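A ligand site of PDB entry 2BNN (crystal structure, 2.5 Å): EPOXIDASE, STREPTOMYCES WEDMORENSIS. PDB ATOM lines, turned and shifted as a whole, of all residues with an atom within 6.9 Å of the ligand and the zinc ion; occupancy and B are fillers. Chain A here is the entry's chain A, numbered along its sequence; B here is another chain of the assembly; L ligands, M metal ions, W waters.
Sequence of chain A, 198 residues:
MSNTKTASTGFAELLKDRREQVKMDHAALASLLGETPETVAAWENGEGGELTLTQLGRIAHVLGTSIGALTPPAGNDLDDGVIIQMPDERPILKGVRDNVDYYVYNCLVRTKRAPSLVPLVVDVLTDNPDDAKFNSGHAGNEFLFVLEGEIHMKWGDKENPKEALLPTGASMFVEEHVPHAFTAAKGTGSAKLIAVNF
An oxygen (O2) of the ligand lies within salt-bridge range of the side-chain amino group (NZ) of Lys 23 of chain B (2.5 Å).
The guanidinium group (NH2) of Arg 97 lies within salt-bridge range of an oxygen (O3) of the ligand, at 2.9 Å.
ND2 of Asn 135 lies within hydrogen-bond range of O3 of the ligand (2.9 Å).
OH of Tyr 105 lies within hydrogen-bond range of O2 of the ligand (3.2 Å).
Asn 135 touches the zinc ion (ND2 to ZN, 3.9 Å).
Four residues have an atom within 4 Å of the zinc ion: Asn 135, His 138, Glu 142 and His 180.
Water W1 lies within hydrogen-bond range of an oxygen (O3) of the ligand (2.5 Å), the backbone carbonyl oxygen of His 180 (2.8 Å), the guanidinium group of Arg 97 (3.0 Å) and the side-chain hydroxyl of Tyr 103 (3.0 Å).
Merely in contact with the ligand: Phe 182, Ala 195 and Leu 120.
Hydrophobic or aromatic side chains that line the ligand: Tyr 105, Leu 120, His 138, His 180, Phe 182 and Ala 195.
The side-chain carboxylate of Glu 142 sits at hydrogen-bond distance from the side-chain amide nitrogen of Asn 197.
N of Val 174 lies within hydrogen-bond range of O of Glu 142 (2.8 Å).
A ring nitrogen (ND1) of His 180 sits at hydrogen-bond distance from the backbone carbonyl oxygen (O) of Val 178, 2.8 Å away.
The side-chain amino group (NZ) of Lys 23 of chain B lies close to the side-chain hydroxyl (OH) of Tyr 105, 3.5 Å away.
The guanidinium group of Arg 97 is in hydrogen-bond range of the backbone carbonyl oxygen of Lys 133 (2.8 Å).
OD1 of Asn 135 sits close to N of Gly 137 (3.4 Å).
The side-chain hydroxyl (OH) of Tyr 103 sits at hydrogen-bond distance from the backbone NH (N) of Phe 182, at 3.2 Å.
The backbone NH (N) of Leu 120 lies within hydrogen-bond range of the backbone carbonyl oxygen (O) of Ala 195.
OE2 of Glu 142 binds the zinc ion, 2.0 Å away.
An oxygen (O4) of the ligand is bound to the zinc ion (2.1 Å).
A ring nitrogen (NE2) of His 180 is bound to the zinc ion, at 2.1 Å.
NE2 of His 138 binds the zinc ion, at 2.2 Å.
Slightly farther from the zinc ion lies an oxygen (O1) of the ligand (2.8 Å).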
ATOM      1  N   ARG A  97      20.379  -5.661   8.905  1.00  0.00           N
ATOM      2  CA  ARG A  97      21.725  -5.472   8.313  1.00  0.00           C
ATOM      3  C   ARG A  97      22.823  -5.148   9.338  1.00  0.00           C
ATOM      4  O   ARG A  97      23.899  -5.781   9.310  1.00  0.00           O
ATOM      5  CB  ARG A  97      21.700  -4.464   7.158  1.00  0.00           C
ATOM      6  CG  ARG A  97      20.718  -4.886   6.056  1.00  0.00           C
ATOM      7  CD  ARG A  97      21.142  -4.532   4.639  1.00  0.00           C
ATOM      8  NE  ARG A  97      20.516  -5.449   3.670  1.00  0.00           N
ATOM      9  CZ  ARG A  97      20.577  -5.308   2.335  1.00  0.00           C
ATOM     10  NH1 ARG A  97      21.221  -4.286   1.784  1.00  0.00           N
ATOM     11  NH2 ARG A  97      19.980  -6.208   1.556  1.00  0.00           N
ATOM     12  N   TYR A 103      14.672  -3.882   6.022  1.00  0.00           N
ATOM     13  CA  TYR A 103      13.640  -4.276   5.073  1.00  0.00           C
ATOM     14  C   TYR A 103      12.663  -5.274   5.692  1.00  0.00           C
ATOM     15  O   TYR A 103      13.023  -6.006   6.620  1.00  0.00           O
ATOM     16  CB  TYR A 103      14.266  -4.951   3.850  1.00  0.00           C
ATOM     17  CG  TYR A 103      15.226  -4.153   2.975  1.00  0.00           C
ATOM     18  CD1 TYR A 103      16.396  -4.743   2.501  1.00  0.00           C
ATOM     19  CD2 TYR A 103      14.940  -2.842   2.592  1.00  0.00           C
ATOM     20  CE1 TYR A 103      17.281  -4.046   1.678  1.00  0.00           C
ATOM     21  CE2 TYR A 103      15.832  -2.121   1.769  1.00  0.00           C
ATOM     22  CZ  TYR A 103      16.997  -2.739   1.304  1.00  0.00           C
ATOM     23  OH  TYR A 103      17.885  -2.052   0.497  1.00  0.00           O
ATOM     24  N   TYR A 105      10.671  -8.320   3.817  1.00  0.00           N
ATOM     25  CA  TYR A 105      10.431  -9.057   2.581  1.00  0.00           C
ATOM     26  C   TYR A 105       9.096  -9.803   2.588  1.00  0.00           C
ATOM     27  O   TYR A 105       8.895 -10.716   3.389  1.00  0.00           O
ATOM     28  CB  TYR A 105      11.547 -10.072   2.360  1.00  0.00           C
ATOM     29  CG  TYR A 105      12.933  -9.482   2.305  1.00  0.00           C
ATOM     30  CD1 TYR A 105      13.844  -9.729   3.331  1.00  0.00           C
ATOM     31  CD2 TYR A 105      13.330  -8.686   1.238  1.00  0.00           C
ATOM     32  CE1 TYR A 105      15.131  -9.181   3.284  1.00  0.00           C
ATOM     33  CE2 TYR A 105      14.601  -8.134   1.185  1.00  0.00           C
ATOM     34  CZ  TYR A 105      15.505  -8.387   2.209  1.00  0.00           C
ATOM     35  OH  TYR A 105      16.768  -7.854   2.147  1.00  0.00           O
ATOM     36  N   VAL A 118      12.607 -14.715  -8.285  1.00  0.00           N
ATOM     37  CA  VAL A 118      12.344 -14.401  -6.881  1.00  0.00           C
ATOM     38  C   VAL A 118      11.751 -12.994  -6.756  1.00  0.00           C
ATOM     39  O   VAL A 118      12.488 -11.988  -6.595  1.00  0.00           O
ATOM     40  CB  VAL A 118      13.604 -14.529  -5.985  1.00  0.00           C
ATOM     41  CG1 VAL A 118      13.227 -14.368  -4.515  1.00  0.00           C
ATOM     42  CG2 VAL A 118      14.329 -15.855  -6.207  1.00  0.00           C
ATOM     43  N   LEU A 120       9.293 -10.010  -4.971  1.00  0.00           N
ATOM     44  CA  LEU A 120       9.051  -9.566  -3.603  1.00  0.00           C
ATOM     45  C   LEU A 120       8.382  -8.197  -3.577  1.00  0.00           C
ATOM     46  O   LEU A 120       8.697  -7.334  -4.394  1.00  0.00           O
ATOM     47  CB  LEU A 120      10.354  -9.405  -2.836  1.00  0.00           C
ATOM     48  CG  LEU A 120      11.498 -10.415  -2.875  1.00  0.00           C
ATOM     49  CD1 LEU A 120      12.817  -9.677  -2.697  1.00  0.00           C
ATOM     50  CD2 LEU A 120      11.304 -11.483  -1.813  1.00  0.00           C
ATOM     51  N   VAL A 122       8.927  -5.390  -1.118  1.00  0.00           N
ATOM     52  CA  VAL A 122       9.908  -5.036  -0.101  1.00  0.00           C
ATOM     53  C   VAL A 122       9.435  -3.778   0.647  1.00  0.00           C
ATOM     54  O   VAL A 122       9.317  -2.711   0.063  1.00  0.00           O
ATOM     55  CB  VAL A 122      11.290  -4.820  -0.765  1.00  0.00           C
ATOM     56  CG1 VAL A 122      12.344  -4.403   0.227  1.00  0.00           C
ATOM     57  CG2 VAL A 122      11.724  -6.076  -1.527  1.00  0.00           C
ATOM     58  N   LYS A 133      22.208   0.891   3.637  1.00  0.00           N
ATOM     59  CA  LYS A 133      23.065  -0.260   3.820  1.00  0.00           C
ATOM     60  C   LYS A 133      23.081  -1.101   2.558  1.00  0.00           C
ATOM     61  O   LYS A 133      22.057  -1.637   2.132  1.00  0.00           O
ATOM     62  CB  LYS A 133      22.625  -1.056   5.045  1.00  0.00           C
ATOM     63  CG  LYS A 133      23.789  -1.517   5.904  1.00  0.00           C
ATOM     64  CD  LYS A 133      23.534  -1.235   7.382  1.00  0.00           C
ATOM     65  CE  LYS A 133      23.844   0.211   7.754  1.00  0.00           C
ATOM     66  NZ  LYS A 133      23.289   0.559   9.096  1.00  0.00           N
ATOM     67  N   PHE A 134      24.271  -1.187   1.963  1.00  0.00           N
ATOM     68  CA  PHE A 134      24.503  -1.891   0.709  1.00  0.00           C
ATOM     69  C   PHE A 134      24.524  -3.398   0.898  1.00  0.00           C
ATOM     70  O   PHE A 134      25.026  -3.899   1.913  1.00  0.00           O
ATOM     71  CB  PHE A 134      25.856  -1.479   0.134  1.00  0.00           C
ATOM     72  CG  PHE A 134      25.821  -0.199  -0.639  1.00  0.00           C
ATOM     73  CD1 PHE A 134      25.797   1.034   0.007  1.00  0.00           C
ATOM     74  CD2 PHE A 134      25.822  -0.237  -2.036  1.00  0.00           C
ATOM     75  CE1 PHE A 134      25.764   2.203  -0.724  1.00  0.00           C
ATOM     76  CE2 PHE A 134      25.793   0.948  -2.782  1.00  0.00           C
ATOM     77  CZ  PHE A 134      25.765   2.166  -2.122  1.00  0.00           C
ATOM     78  N   ASN A 135      24.003  -4.137  -0.074  1.00  0.00           N
ATOM     79  CA  ASN A 135      24.374  -5.534  -0.195  1.00  0.00           C
ATOM     80  C   ASN A 135      25.711  -5.565  -0.963  1.00  0.00           C
ATOM     81  O   ASN A 135      26.309  -4.511  -1.187  1.00  0.00           O
ATOM     82  CB  ASN A 135      23.274  -6.354  -0.890  1.00  0.00           C
ATOM     83  CG  ASN A 135      22.825  -5.771  -2.217  1.00  0.00           C
ATOM     84  OD1 ASN A 135      23.469  -4.872  -2.778  1.00  0.00           O
ATOM     85  ND2 ASN A 135      21.724  -6.293  -2.748  1.00  0.00           N
ATOM     86  N   GLY A 137      25.879  -6.888  -3.990  1.00  0.00           N
ATOM     87  CA  GLY A 137      25.348  -7.378  -5.264  1.00  0.00           C
ATOM     88  C   GLY A 137      24.935  -8.831  -5.121  1.00  0.00           C
ATOM     89  O   GLY A 137      25.410  -9.516  -4.225  1.00  0.00           O
ATOM     90  N   HIS A 138      24.054  -9.299  -6.001  1.00  0.00           N
ATOM     91  CA  HIS A 138      23.651 -10.704  -5.950  1.00  0.00           C
ATOM     92  C   HIS A 138      23.557 -11.364  -7.323  1.00  0.00           C
ATOM     93  O   HIS A 138      23.726 -10.689  -8.352  1.00  0.00           O
ATOM     94  CB  HIS A 138      22.355 -10.910  -5.135  1.00  0.00           C
ATOM     95  CG  HIS A 138      21.306  -9.873  -5.389  1.00  0.00           C
ATOM     96  ND1 HIS A 138      20.790  -9.615  -6.639  1.00  0.00           N
ATOM     97  CD2 HIS A 138      20.672  -9.027  -4.534  1.00  0.00           C
ATOM     98  CE1 HIS A 138      19.888  -8.654  -6.547  1.00  0.00           C
ATOM     99  NE2 HIS A 138      19.792  -8.287  -5.285  1.00  0.00           N
ATOM    100  N   GLY A 140      21.231 -12.812  -9.356  1.00  0.00           N
ATOM    101  CA  GLY A 140      20.281 -12.567 -10.434  1.00  0.00           C
ATOM    102  C   GLY A 140      20.318 -11.133 -10.964  1.00  0.00           C
ATOM    103  O   GLY A 140      20.794 -10.216 -10.290  1.00  0.00           O
ATOM    104  N   GLU A 142      17.903  -7.963 -11.700  1.00  0.00           N
ATOM    105  CA  GLU A 142      16.757  -7.499 -10.918  1.00  0.00           C
ATOM    106  C   GLU A 142      15.939  -6.352 -11.539  1.00  0.00           C
ATOM    107  O   GLU A 142      16.482  -5.282 -11.860  1.00  0.00           O
ATOM    108  CB  GLU A 142      17.202  -7.141  -9.502  1.00  0.00           C
ATOM    109  CG  GLU A 142      16.071  -7.149  -8.484  1.00  0.00           C
ATOM    110  CD  GLU A 142      16.600  -7.236  -7.075  1.00  0.00           C
ATOM    111  OE1 GLU A 142      16.441  -8.307  -6.437  1.00  0.00           O
ATOM    112  OE2 GLU A 142      17.192  -6.247  -6.615  1.00  0.00           O
ATOM    113  N   LEU A 144      12.870  -3.647 -10.746  1.00  0.00           N
ATOM    114  CA  LEU A 144      12.284  -3.001  -9.582  1.00  0.00           C
ATOM    115  C   LEU A 144      11.318  -1.912  -9.963  1.00  0.00           C
ATOM    116  O   LEU A 144      11.506  -1.233 -10.971  1.00  0.00           O
ATOM    117  CB  LEU A 144      13.338  -2.405  -8.655  1.00  0.00           C
ATOM    118  CG  LEU A 144      14.307  -3.400  -8.026  1.00  0.00           C
ATOM    119  CD1 LEU A 144      15.708  -3.194  -8.631  1.00  0.00           C
ATOM    120  CD2 LEU A 144      14.308  -3.248  -6.497  1.00  0.00           C
ATOM    121  N   VAL A 174      18.615  -3.549 -12.178  1.00  0.00           N
ATOM    122  CA  VAL A 174      19.950  -3.729 -11.604  1.00  0.00           C
ATOM    123  C   VAL A 174      20.569  -5.030 -12.115  1.00  0.00           C
ATOM    124  O   VAL A 174      20.062  -6.114 -11.833  1.00  0.00           O
ATOM    125  CB  VAL A 174      19.958  -3.702 -10.052  1.00  0.00           C
ATOM    126  CG1 VAL A 174      21.372  -3.914  -9.522  1.00  0.00           C
ATOM    127  CG2 VAL A 174      19.420  -2.392  -9.528  1.00  0.00           C
ATOM    128  N   VAL A 178      25.900  -6.192  -9.271  1.00  0.00           N
ATOM    129  CA  VAL A 178      25.981  -4.769  -8.971  1.00  0.00           C
ATOM    130  C   VAL A 178      25.431  -4.495  -7.566  1.00  0.00           C
ATOM    131  O   VAL A 178      24.281  -4.835  -7.281  1.00  0.00           O
ATOM    132  CB  VAL A 178      25.225  -3.913 -10.007  1.00  0.00           C
ATOM    133  CG1 VAL A 178      25.148  -2.448  -9.548  1.00  0.00           C
ATOM    134  CG2 VAL A 178      25.880  -4.010 -11.370  1.00  0.00           C
ATOM    135  N   HIS A 180      23.860  -2.557  -4.377  1.00  0.00           N
ATOM    136  CA  HIS A 180      22.819  -1.526  -4.288  1.00  0.00           C
ATOM    137  C   HIS A 180      22.120  -1.442  -2.924  1.00  0.00           C
ATOM    138  O   HIS A 180      22.014  -2.430  -2.194  1.00  0.00           O
ATOM    139  CB  HIS A 180      21.770  -1.728  -5.384  1.00  0.00           C
ATOM    140  CG  HIS A 180      21.227  -3.126  -5.428  1.00  0.00           C
ATOM    141  ND1 HIS A 180      21.915  -4.171  -6.009  1.00  0.00           N
ATOM    142  CD2 HIS A 180      20.085  -3.655  -4.924  1.00  0.00           C
ATOM    143  CE1 HIS A 180      21.214  -5.280  -5.876  1.00  0.00           C
ATOM    144  NE2 HIS A 180      20.103  -4.988  -5.230  1.00  0.00           N
ATOM    145  N   ALA A 181      21.639  -0.246  -2.602  1.00  0.00           N
ATOM    146  CA  ALA A 181      20.939   0.017  -1.347  1.00  0.00           C
ATOM    147  C   ALA A 181      19.727   0.897  -1.597  1.00  0.00           C
ATOM    148  O   ALA A 181      19.730   1.715  -2.504  1.00  0.00           O
ATOM    149  CB  ALA A 181      21.891   0.664  -0.348  1.00  0.00           C
ATOM    150  N   PHE A 182      18.698   0.736  -0.775  1.00  0.00           N
ATOM    151  CA  PHE A 182      17.513   1.562  -0.852  1.00  0.00           C
ATOM    152  C   PHE A 182      17.124   2.045   0.542  1.00  0.00           C
ATOM    153  O   PHE A 182      17.262   1.292   1.515  1.00  0.00           O
ATOM    154  CB  PHE A 182      16.326   0.768  -1.399  1.00  0.00           C
ATOM    155  CG  PHE A 182      16.569   0.081  -2.703  1.00  0.00           C
ATOM    156  CD1 PHE A 182      16.803  -1.288  -2.747  1.00  0.00           C
ATOM    157  CD2 PHE A 182      16.531   0.804  -3.908  1.00  0.00           C
ATOM    158  CE1 PHE A 182      17.031  -1.932  -3.978  1.00  0.00           C
ATOM    159  CE2 PHE A 182      16.745   0.160  -5.136  1.00  0.00           C
ATOM    160  CZ  PHE A 182      17.002  -1.208  -5.172  1.00  0.00           C
ATOM    161  N   LEU A 193       8.810  -1.391  -2.539  1.00  0.00           N
ATOM    162  CA  LEU A 193       9.318  -1.840  -3.834  1.00  0.00           C
ATOM    163  C   LEU A 193       8.627  -3.128  -4.229  1.00  0.00           C
ATOM    164  O   LEU A 193       8.333  -3.963  -3.378  1.00  0.00           O
ATOM    165  CB  LEU A 193      10.817  -2.104  -3.766  1.00  0.00           C
ATOM    166  CG  LEU A 193      11.745  -0.907  -3.572  1.00  0.00           C
ATOM    167  CD1 LEU A 193      13.170  -1.377  -3.268  1.00  0.00           C
ATOM    168  CD2 LEU A 193      11.729   0.018  -4.799  1.00  0.00           C
ATOM    169  N   ALA A 195      10.281  -5.989  -6.146  1.00  0.00           N
ATOM    170  CA  ALA A 195      11.560  -6.419  -6.681  1.00  0.00           C
ATOM    171  C   ALA A 195      11.334  -7.758  -7.359  1.00  0.00           C
ATOM    172  O   ALA A 195      10.691  -8.645  -6.791  1.00  0.00           O
ATOM    173  CB  ALA A 195      12.571  -6.554  -5.579  1.00  0.00           C
ATOM    174  N   VAL A 196      11.850  -7.890  -8.586  1.00  0.00           N
ATOM    175  CA  VAL A 196      11.777  -9.163  -9.292  1.00  0.00           C
ATOM    176  C   VAL A 196      13.166  -9.604  -9.704  1.00  0.00           C
ATOM    177  O   VAL A 196      13.763  -9.066 -10.651  1.00  0.00           O
ATOM    178  CB  VAL A 196      10.849  -9.112 -10.492  1.00  0.00           C
ATOM    179  CG1 VAL A 196      10.755 -10.498 -11.163  1.00  0.00           C
ATOM    180  CG2 VAL A 196       9.456  -8.598 -10.097  1.00  0.00           C
ATOM    181  N   ASN A 197      13.702 -10.566  -8.961  1.00  0.00           N
ATOM    182  CA  ASN A 197      14.992 -11.131  -9.259  1.00  0.00           C
ATOM    183  C   ASN A 197      14.734 -12.257 -10.242  1.00  0.00           C
ATOM    184  O   ASN A 197      13.810 -13.059 -10.046  1.00  0.00           O
ATOM    185  CB  ASN A 197      15.652 -11.648  -7.984  1.00  0.00           C
ATOM    186  CG  ASN A 197      17.169 -11.691  -8.077  1.00  0.00           C
ATOM    187  OD1 ASN A 197      17.768 -12.764  -8.030  1.00  0.00           O
ATOM    188  ND2 ASN A 197      17.797 -10.527  -8.211  1.00  0.00           N
ATOM    189  N   LYS B  23      15.564 -15.315   0.579  1.00  0.00           N
ATOM    190  CA  LYS B  23      15.318 -14.522   1.803  1.00  0.00           C
ATOM    191  C   LYS B  23      15.125 -15.304   3.114  1.00  0.00           C
ATOM    192  O   LYS B  23      14.726 -14.705   4.123  1.00  0.00           O
ATOM    193  CB  LYS B  23      14.154 -13.544   1.620  1.00  0.00           C
ATOM    194  CG  LYS B  23      14.325 -12.546   0.513  1.00  0.00           C
ATOM    195  CD  LYS B  23      15.602 -11.749   0.661  1.00  0.00           C
ATOM    196  CE  LYS B  23      16.086 -11.311  -0.699  1.00  0.00           C
ATOM    197  NZ  LYS B  23      16.836 -10.046  -0.560  1.00  0.00           N
HETATM  198  C1  LIG L   1      16.891  -5.298  -2.194  1.00  0.00           C
HETATM  199  C2  LIG L   1      15.631  -5.646  -2.980  1.00  0.00           C
HETATM  200  C3  LIG L   1      15.515  -7.098  -3.463  1.00  0.00           C
HETATM  201  O1  LIG L   1      16.780  -5.060  -3.593  1.00  0.00           O
HETATM  202  P1  LIG L   1      18.024  -6.683  -1.904  1.00  0.00           P
HETATM  203  O2  LIG L   1      17.235  -7.594  -1.009  1.00  0.00           O
HETATM  204  O3  LIG L   1      19.228  -6.054  -1.243  1.00  0.00           O
HETATM  205  O4  LIG L   1      18.362  -7.299  -3.234  1.00  0.00           O
HETATM  206 ZN    ZN M   1      18.599  -6.475  -5.145  1.00  0.00          ZN
HETATM  207  O   HOH W   1      19.982  -3.730  -0.860  1.00  0.00           O
